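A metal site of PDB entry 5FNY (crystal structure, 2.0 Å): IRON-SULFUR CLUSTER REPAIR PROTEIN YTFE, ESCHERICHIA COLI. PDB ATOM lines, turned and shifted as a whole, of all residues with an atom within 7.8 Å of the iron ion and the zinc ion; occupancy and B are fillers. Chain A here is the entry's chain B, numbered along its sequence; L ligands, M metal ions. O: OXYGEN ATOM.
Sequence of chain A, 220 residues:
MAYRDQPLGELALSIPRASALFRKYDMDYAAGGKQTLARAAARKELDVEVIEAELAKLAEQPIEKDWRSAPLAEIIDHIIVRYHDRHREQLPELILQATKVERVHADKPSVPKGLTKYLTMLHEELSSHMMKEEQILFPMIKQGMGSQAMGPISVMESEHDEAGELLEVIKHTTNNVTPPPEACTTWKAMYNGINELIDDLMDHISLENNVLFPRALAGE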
ATOM      1  N   ILE A  79     -19.575 -20.879  -1.336  1.00  0.00           N
ATOM      2  CA  ILE A  79     -19.871 -22.330  -1.282  1.00  0.00           C
ATOM      3  C   ILE A  79     -20.738 -22.769  -2.469  1.00  0.00           C
ATOM      4  O   ILE A  79     -20.442 -23.764  -3.128  1.00  0.00           O
ATOM      5  CB  ILE A  79     -20.552 -22.720   0.044  1.00  0.00           C
ATOM      6  CG1 ILE A  79     -19.535 -22.677   1.169  1.00  0.00           C
ATOM      7  CG2 ILE A  79     -21.196 -24.112  -0.053  1.00  0.00           C
ATOM      8  CD1 ILE A  79     -20.126 -22.724   2.567  1.00  0.00           C
ATOM      9  N   ILE A  80     -21.781 -21.986  -2.738  1.00  0.00           N
ATOM     10  CA  ILE A  80     -22.729 -22.310  -3.785  1.00  0.00           C
ATOM     11  C   ILE A  80     -22.025 -22.363  -5.150  1.00  0.00           C
ATOM     12  O   ILE A  80     -22.222 -23.322  -5.922  1.00  0.00           O
ATOM     13  CB  ILE A  80     -23.960 -21.363  -3.775  1.00  0.00           C
ATOM     14  CG1 ILE A  80     -24.775 -21.605  -2.520  1.00  0.00           C
ATOM     15  CG2 ILE A  80     -24.841 -21.631  -4.994  1.00  0.00           C
ATOM     16  CD1 ILE A  80     -25.798 -20.533  -2.215  1.00  0.00           C
ATOM     17  N   TYR A  83     -18.297 -24.726  -4.906  1.00  0.00           N
ATOM     18  CA  TYR A  83     -18.459 -26.114  -4.503  1.00  0.00           C
ATOM     19  C   TYR A  83     -19.764 -26.736  -4.975  1.00  0.00           C
ATOM     20  O   TYR A  83     -19.706 -27.704  -5.734  1.00  0.00           O
ATOM     21  CB  TYR A  83     -18.223 -26.273  -2.977  1.00  0.00           C
ATOM     22  CG  TYR A  83     -16.797 -25.900  -2.568  1.00  0.00           C
ATOM     23  CD1 TYR A  83     -15.697 -26.574  -3.103  1.00  0.00           C
ATOM     24  CD2 TYR A  83     -16.545 -24.846  -1.689  1.00  0.00           C
ATOM     25  CE1 TYR A  83     -14.404 -26.217  -2.777  1.00  0.00           C
ATOM     26  CE2 TYR A  83     -15.254 -24.492  -1.348  1.00  0.00           C
ATOM     27  CZ  TYR A  83     -14.177 -25.178  -1.902  1.00  0.00           C
ATOM     28  OH  TYR A  83     -12.908 -24.824  -1.572  1.00  0.00           O
ATOM     29  N   HIS A  84     -20.916 -26.240  -4.524  1.00  0.00           N
ATOM     30  CA  HIS A  84     -22.213 -26.905  -4.864  1.00  0.00           C
ATOM     31  C   HIS A  84     -22.365 -27.060  -6.374  1.00  0.00           C
ATOM     32  O   HIS A  84     -22.599 -28.162  -6.870  1.00  0.00           O
ATOM     33  CB  HIS A  84     -23.403 -26.148  -4.296  1.00  0.00           C
ATOM     34  CG  HIS A  84     -23.579 -26.298  -2.827  1.00  0.00           C
ATOM     35  ND1 HIS A  84     -24.765 -26.017  -2.191  1.00  0.00           N
ATOM     36  CD2 HIS A  84     -22.719 -26.682  -1.852  1.00  0.00           C
ATOM     37  CE1 HIS A  84     -24.644 -26.238  -0.902  1.00  0.00           C
ATOM     38  NE2 HIS A  84     -23.416 -26.621  -0.665  1.00  0.00           N
ATOM     39  N   HIS A  87     -19.793 -29.543  -7.866  1.00  0.00           N
ATOM     40  CA  HIS A  87     -20.220 -30.944  -7.681  1.00  0.00           C
ATOM     41  C   HIS A  87     -21.306 -31.385  -8.654  1.00  0.00           C
ATOM     42  O   HIS A  87     -21.298 -32.520  -9.086  1.00  0.00           O
ATOM     43  CB  HIS A  87     -20.728 -31.177  -6.269  1.00  0.00           C
ATOM     44  CG  HIS A  87     -19.725 -30.926  -5.198  1.00  0.00           C
ATOM     45  ND1 HIS A  87     -18.369 -31.046  -5.416  1.00  0.00           N
ATOM     46  CD2 HIS A  87     -19.872 -30.557  -3.917  1.00  0.00           C
ATOM     47  CE1 HIS A  87     -17.717 -30.769  -4.300  1.00  0.00           C
ATOM     48  NE2 HIS A  87     -18.611 -30.487  -3.373  1.00  0.00           N
ATOM     49  N   LEU A 126     -25.941 -35.950  -2.135  1.00  0.00           N
ATOM     50  CA  LEU A 126     -25.463 -34.591  -2.278  1.00  0.00           C
ATOM     51  C   LEU A 126     -26.525 -33.664  -2.836  1.00  0.00           C
ATOM     52  O   LEU A 126     -26.675 -32.564  -2.339  1.00  0.00           O
ATOM     53  CB  LEU A 126     -24.230 -34.502  -3.167  1.00  0.00           C
ATOM     54  CG  LEU A 126     -22.874 -34.693  -2.481  1.00  0.00           C
ATOM     55  CD1 LEU A 126     -21.787 -34.513  -3.537  1.00  0.00           C
ATOM     56  CD2 LEU A 126     -22.703 -33.688  -1.352  1.00  0.00           C
ATOM     57  N   HIS A 129     -29.122 -32.911  -0.153  1.00  0.00           N
ATOM     58  CA  HIS A 129     -28.426 -32.162   0.877  1.00  0.00           C
ATOM     59  C   HIS A 129     -28.188 -30.681   0.483  1.00  0.00           C
ATOM     60  O   HIS A 129     -28.495 -29.763   1.258  1.00  0.00           O
ATOM     61  CB  HIS A 129     -27.098 -32.819   1.183  1.00  0.00           C
ATOM     62  CG  HIS A 129     -26.276 -32.084   2.174  1.00  0.00           C
ATOM     63  ND1 HIS A 129     -26.440 -32.216   3.532  1.00  0.00           N
ATOM     64  CD2 HIS A 129     -25.289 -31.185   1.992  1.00  0.00           C
ATOM     65  CE1 HIS A 129     -25.573 -31.429   4.147  1.00  0.00           C
ATOM     66  NE2 HIS A 129     -24.861 -30.798   3.231  1.00  0.00           N
ATOM     67  N   MET A 130     -27.683 -30.470  -0.725  1.00  0.00           N
ATOM     68  CA  MET A 130     -27.355 -29.116  -1.187  1.00  0.00           C
ATOM     69  C   MET A 130     -28.620 -28.287  -1.401  1.00  0.00           C
ATOM     70  O   MET A 130     -28.608 -27.068  -1.227  1.00  0.00           O
ATOM     71  CB  MET A 130     -26.518 -29.152  -2.470  1.00  0.00           C
ATOM     72  CG  MET A 130     -25.146 -29.727  -2.254  1.00  0.00           C
ATOM     73  SD  MET A 130     -24.065 -29.739  -3.701  1.00  0.00           S
ATOM     74  CE  MET A 130     -25.029 -30.548  -4.972  1.00  0.00           C
ATOM     75  N   MET A 131     -29.723 -28.947  -1.769  1.00  0.00           N
ATOM     76  CA  MET A 131     -31.001 -28.240  -1.889  1.00  0.00           C
ATOM     77  C   MET A 131     -31.564 -27.816  -0.543  1.00  0.00           C
ATOM     78  O   MET A 131     -32.030 -26.710  -0.447  1.00  0.00           O
ATOM     79  CB  MET A 131     -32.034 -29.017  -2.708  1.00  0.00           C
ATOM     80  CG  MET A 131     -31.872 -28.767  -4.199  1.00  0.00           C
ATOM     81  SD  MET A 131     -32.189 -27.050  -4.738  1.00  0.00           S
ATOM     82  CE  MET A 131     -30.630 -26.403  -5.258  1.00  0.00           C
ATOM     83  N   GLU A 133     -29.741 -27.011   2.065  1.00  0.00           N
ATOM     84  CA  GLU A 133     -28.871 -25.904   2.422  1.00  0.00           C
ATOM     85  C   GLU A 133     -29.297 -24.659   1.667  1.00  0.00           C
ATOM     86  O   GLU A 133     -29.595 -23.662   2.290  1.00  0.00           O
ATOM     87  CB  GLU A 133     -27.393 -26.217   2.173  1.00  0.00           C
ATOM     88  CG  GLU A 133     -26.749 -26.997   3.321  1.00  0.00           C
ATOM     89  CD  GLU A 133     -25.316 -27.455   3.058  1.00  0.00           C
ATOM     90  OE1 GLU A 133     -24.811 -27.320   1.910  1.00  0.00           O
ATOM     91  OE2 GLU A 133     -24.690 -27.946   4.020  1.00  0.00           O
ATOM     92  N   GLU A 134     -29.368 -24.735   0.351  1.00  0.00           N
ATOM     93  CA  GLU A 134     -29.605 -23.565  -0.490  1.00  0.00           C
ATOM     94  C   GLU A 134     -31.003 -22.973  -0.302  1.00  0.00           C
ATOM     95  O   GLU A 134     -31.153 -21.761  -0.255  1.00  0.00           O
ATOM     96  CB  GLU A 134     -29.356 -23.875  -1.988  1.00  0.00           C
ATOM     97  CG  GLU A 134     -27.887 -24.082  -2.301  1.00  0.00           C
ATOM     98  CD  GLU A 134     -27.614 -24.585  -3.720  1.00  0.00           C
ATOM     99  OE1 GLU A 134     -28.428 -24.367  -4.637  1.00  0.00           O
ATOM    100  OE2 GLU A 134     -26.561 -25.223  -3.930  1.00  0.00           O
ATOM    101  N   LEU A 137     -31.682 -23.697   4.910  1.00  0.00           N
ATOM    102  CA  LEU A 137     -30.726 -23.343   5.955  1.00  0.00           C
ATOM    103  C   LEU A 137     -29.886 -22.098   5.640  1.00  0.00           C
ATOM    104  O   LEU A 137     -29.767 -21.230   6.489  1.00  0.00           O
ATOM    105  CB  LEU A 137     -29.832 -24.531   6.295  1.00  0.00           C
ATOM    106  CG  LEU A 137     -28.817 -24.301   7.414  1.00  0.00           C
ATOM    107  CD1 LEU A 137     -29.506 -23.953   8.742  1.00  0.00           C
ATOM    108  CD2 LEU A 137     -27.931 -25.514   7.584  1.00  0.00           C
ATOM    109  N   PHE A 138     -29.322 -22.017   4.447  1.00  0.00           N
ATOM    110  CA  PHE A 138     -28.469 -20.845   4.121  1.00  0.00           C
ATOM    111  C   PHE A 138     -29.232 -19.494   4.174  1.00  0.00           C
ATOM    112  O   PHE A 138     -28.705 -18.535   4.722  1.00  0.00           O
ATOM    113  CB  PHE A 138     -27.774 -20.999   2.768  1.00  0.00           C
ATOM    114  CG  PHE A 138     -26.626 -22.018   2.723  1.00  0.00           C
ATOM    115  CD1 PHE A 138     -26.108 -22.628   3.863  1.00  0.00           C
ATOM    116  CD2 PHE A 138     -26.060 -22.333   1.488  1.00  0.00           C
ATOM    117  CE1 PHE A 138     -25.032 -23.522   3.765  1.00  0.00           C
ATOM    118  CE2 PHE A 138     -24.995 -23.221   1.383  1.00  0.00           C
ATOM    119  CZ  PHE A 138     -24.482 -23.822   2.524  1.00  0.00           C
ATOM    120  N   MET A 156     -27.365 -31.403   9.365  1.00  0.00           N
ATOM    121  CA  MET A 156     -26.485 -31.225   8.222  1.00  0.00           C
ATOM    122  C   MET A 156     -25.103 -31.833   8.491  1.00  0.00           C
ATOM    123  O   MET A 156     -24.503 -32.418   7.598  1.00  0.00           O
ATOM    124  CB  MET A 156     -26.325 -29.747   7.855  1.00  0.00           C
ATOM    125  CG  MET A 156     -27.618 -29.080   7.425  1.00  0.00           C
ATOM    126  SD  MET A 156     -28.381 -29.758   5.938  1.00  0.00           S
ATOM    127  CE  MET A 156     -29.560 -30.901   6.586  1.00  0.00           C
ATOM    128  N   GLU A 157     -24.608 -31.723   9.721  1.00  0.00           N
ATOM    129  CA  GLU A 157     -23.317 -32.310  10.042  1.00  0.00           C
ATOM    130  C   GLU A 157     -23.383 -33.838  10.058  1.00  0.00           C
ATOM    131  O   GLU A 157     -22.423 -34.493   9.654  1.00  0.00           O
ATOM    132  CB  GLU A 157     -22.747 -31.735  11.340  1.00  0.00           C
ATOM    133  CG  GLU A 157     -22.435 -30.245  11.215  1.00  0.00           C
ATOM    134  CD  GLU A 157     -21.563 -29.679  12.336  1.00  0.00           C
ATOM    135  OE1 GLU A 157     -21.535 -30.259  13.449  1.00  0.00           O
ATOM    136  OE2 GLU A 157     -20.909 -28.628  12.113  1.00  0.00           O
ATOM    137  N   GLU A 159     -25.357 -35.484   7.997  1.00  0.00           N
ATOM    138  CA  GLU A 159     -25.346 -35.770   6.570  1.00  0.00           C
ATOM    139  C   GLU A 159     -23.937 -35.669   5.969  1.00  0.00           C
ATOM    140  O   GLU A 159     -23.571 -36.460   5.105  1.00  0.00           O
ATOM    141  CB  GLU A 159     -26.346 -34.869   5.820  1.00  0.00           C
ATOM    142  CG  GLU A 159     -27.803 -35.225   6.174  1.00  0.00           C
ATOM    143  CD  GLU A 159     -28.858 -34.501   5.318  1.00  0.00           C
ATOM    144  OE1 GLU A 159     -28.516 -33.677   4.421  1.00  0.00           O
ATOM    145  OE2 GLU A 159     -30.059 -34.771   5.556  1.00  0.00           O
ATOM    146  N   HIS A 160     -23.150 -34.692   6.418  1.00  0.00           N
ATOM    147  CA  HIS A 160     -21.727 -34.624   6.015  1.00  0.00           C
ATOM    148  C   HIS A 160     -20.965 -35.897   6.392  1.00  0.00           C
ATOM    149  O   HIS A 160     -20.216 -36.409   5.578  1.00  0.00           O
ATOM    150  CB  HIS A 160     -21.038 -33.407   6.650  1.00  0.00           C
ATOM    151  CG  HIS A 160     -21.545 -32.104   6.126  1.00  0.00           C
ATOM    152  ND1 HIS A 160     -21.250 -30.902   6.724  1.00  0.00           N
ATOM    153  CD2 HIS A 160     -22.339 -31.800   5.058  1.00  0.00           C
ATOM    154  CE1 HIS A 160     -21.813 -29.915   6.049  1.00  0.00           C
ATOM    155  NE2 HIS A 160     -22.489 -30.440   5.035  1.00  0.00           N
ATOM    156  N   LEU A 201     -14.782 -31.801  -2.065  1.00  0.00           N
ATOM    157  CA  LEU A 201     -15.793 -32.150  -1.092  1.00  0.00           C
ATOM    158  C   LEU A 201     -15.274 -31.959   0.320  1.00  0.00           C
ATOM    159  O   LEU A 201     -16.006 -31.453   1.185  1.00  0.00           O
ATOM    160  CB  LEU A 201     -16.280 -33.585  -1.337  1.00  0.00           C
ATOM    161  CG  LEU A 201     -17.610 -34.069  -0.781  1.00  0.00           C
ATOM    162  CD1 LEU A 201     -18.693 -32.990  -0.820  1.00  0.00           C
ATOM    163  CD2 LEU A 201     -18.017 -35.299  -1.568  1.00  0.00           C
ATOM    164  N   HIS A 204     -15.030 -28.158   0.908  1.00  0.00           N
ATOM    165  CA  HIS A 204     -16.427 -27.713   1.029  1.00  0.00           C
ATOM    166  C   HIS A 204     -16.946 -28.022   2.436  1.00  0.00           C
ATOM    167  O   HIS A 204     -17.403 -27.134   3.168  1.00  0.00           O
ATOM    168  CB  HIS A 204     -17.232 -28.402  -0.097  1.00  0.00           C
ATOM    169  CG  HIS A 204     -18.718 -28.317   0.007  1.00  0.00           C
ATOM    170  ND1 HIS A 204     -19.533 -29.182  -0.680  1.00  0.00           N
ATOM    171  CD2 HIS A 204     -19.539 -27.536   0.748  1.00  0.00           C
ATOM    172  CE1 HIS A 204     -20.803 -28.933  -0.396  1.00  0.00           C
ATOM    173  NE2 HIS A 204     -20.820 -27.952   0.493  1.00  0.00           N
ATOM    174  N   ILE A 205     -16.877 -29.278   2.834  1.00  0.00           N
ATOM    175  CA  ILE A 205     -17.383 -29.677   4.148  1.00  0.00           C
ATOM    176  C   ILE A 205     -16.583 -29.012   5.248  1.00  0.00           C
ATOM    177  O   ILE A 205     -17.156 -28.626   6.306  1.00  0.00           O
ATOM    178  CB  ILE A 205     -17.388 -31.206   4.322  1.00  0.00           C
ATOM    179  CG1 ILE A 205     -18.401 -31.841   3.398  1.00  0.00           C
ATOM    180  CG2 ILE A 205     -17.705 -31.629   5.768  1.00  0.00           C
ATOM    181  CD1 ILE A 205     -18.167 -33.323   3.245  1.00  0.00           C
ATOM    182  N   GLU A 208     -17.860 -25.519   5.752  1.00  0.00           N
ATOM    183  CA  GLU A 208     -19.132 -25.537   6.497  1.00  0.00           C
ATOM    184  C   GLU A 208     -18.971 -25.915   7.967  1.00  0.00           C
ATOM    185  O   GLU A 208     -19.379 -25.139   8.838  1.00  0.00           O
ATOM    186  CB  GLU A 208     -20.143 -26.439   5.776  1.00  0.00           C
ATOM    187  CG  GLU A 208     -20.521 -25.875   4.413  1.00  0.00           C
ATOM    188  CD  GLU A 208     -21.545 -26.685   3.647  1.00  0.00           C
ATOM    189  OE1 GLU A 208     -21.977 -27.743   4.159  1.00  0.00           O
ATOM    190  OE2 GLU A 208     -21.937 -26.246   2.515  1.00  0.00           O
ATOM    191  N   ASN A 209     -18.314 -27.043   8.233  1.00  0.00           N
ATOM    192  CA  ASN A 209     -18.144 -27.571   9.607  1.00  0.00           C
ATOM    193  C   ASN A 209     -17.215 -26.761  10.507  1.00  0.00           C
ATOM    194  O   ASN A 209     -17.413 -26.710  11.696  1.00  0.00           O
ATOM    195  CB  ASN A 209     -17.619 -29.015   9.600  1.00  0.00           C
ATOM    196  CG  ASN A 209     -18.703 -30.035   9.291  1.00  0.00           C
ATOM    197  OD1 ASN A 209     -19.785 -29.674   8.857  1.00  0.00           O
ATOM    198  ND2 ASN A 209     -18.406 -31.297   9.497  1.00  0.00           N
ATOM    199  N   LEU A 212     -18.428 -21.842   8.760  1.00  0.00           N
ATOM    200  CA  LEU A 212     -19.790 -21.317   8.638  1.00  0.00           C
ATOM    201  C   LEU A 212     -20.660 -21.693   9.823  1.00  0.00           C
ATOM    202  O   LEU A 212     -21.298 -20.823  10.433  1.00  0.00           O
ATOM    203  CB  LEU A 212     -20.452 -21.786   7.354  1.00  0.00           C
ATOM    204  CG  LEU A 212     -21.863 -21.227   7.045  1.00  0.00           C
ATOM    205  CD1 LEU A 212     -21.845 -19.717   6.783  1.00  0.00           C
ATOM    206  CD2 LEU A 212     -22.457 -21.969   5.862  1.00  0.00           C
ATOM    207  N   PHE A 213     -20.767 -22.987  10.088  1.00  0.00           N
ATOM    208  CA  PHE A 213     -21.682 -23.449  11.133  1.00  0.00           C
ATOM    209  C   PHE A 213     -21.274 -22.982  12.519  1.00  0.00           C
ATOM    210  O   PHE A 213     -22.142 -22.514  13.262  1.00  0.00           O
ATOM    211  CB  PHE A 213     -21.893 -24.956  11.100  1.00  0.00           C
ATOM    212  CG  PHE A 213     -22.569 -25.484   9.855  1.00  0.00           C
ATOM    213  CD1 PHE A 213     -23.276 -24.660   8.967  1.00  0.00           C
ATOM    214  CD2 PHE A 213     -22.519 -26.855   9.578  1.00  0.00           C
ATOM    215  CE1 PHE A 213     -23.875 -25.186   7.831  1.00  0.00           C
ATOM    216  CE2 PHE A 213     -23.148 -27.376   8.447  1.00  0.00           C
ATOM    217  CZ  PHE A 213     -23.827 -26.537   7.585  1.00  0.00           C
HETATM  218  O     O L   1     -22.866 -29.236   1.456  1.00  0.00           O
HETATM  219 FE    FE M   1     -22.781 -27.493   1.167  1.00  0.00          FE
HETATM  220 ZN    ZN M   2     -23.388 -29.353   3.577  1.00  0.00          ZN
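The side-chain carboxylate (OE2) of Glu 133 is bound to the zinc ion.
NE2 of His 160 binds the zinc ion (2.0 Å).
NE2 of His 129 binds the zinc ion.
The zinc ion is bound by O of the ligand, 2.2 Å away.
The zinc ion is bound by OE1 of Glu 208 (2.2 Å).
The zinc ion has five donor atoms within binding distance.
Within 4 Å of the zinc ion: His 129, Glu 133, His 160 and Glu 208.
The nearest printed residue that does not touch the zinc ion is His 204 (4.3 Å).
Ile 79 touches the iron ion (CG2 to FE, 3.9 Å).
Within 4 Å of the iron ion: Ile 79, His 84, Glu 133, His 204 and Glu 208.
The iron ion is bound by an oxygen (O) of the ligand (1.8 Å), the side-chain carboxylate (OE2) of Glu 208 (2.0 Å), a ring nitrogen (NE2) of His 204 (2.1 Å), a ring nitrogen (NE2) of His 84 (2.1 Å) and the side-chain carboxylate (OE1) of Glu 133 (2.2 Å).
The iron ion has five donor atoms within binding distance.
The backbone NH (N) of Phe 138 is in hydrogen-bond range of the backbone carbonyl oxygen (O) of Glu 133 (2.7 Å).
N of Phe 213 sits at hydrogen-bond distance from O of Glu 208 (2.8 Å).
OD1 of Asn 209 is in hydrogen-bond range of ND1 of His 160 (2.9 Å).
A ring nitrogen (ND1) of His 129 lies within hydrogen-bond range of the side-chain carboxylate (OE1) of Glu 159 (2.7 Å).
A ring nitrogen (ND1) of His 204 is in hydrogen-bond range of a ring nitrogen (NE2) of His 87 (3.1 Å).
The backbone carbonyl oxygen (O) of Ile 79 is in hydrogen-bond range of the backbone NH (N) of His 84 (2.9 Å).
OE2 of Glu 134 is in hydrogen-bond range of ND1 of His 84, at 2.6 Å.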
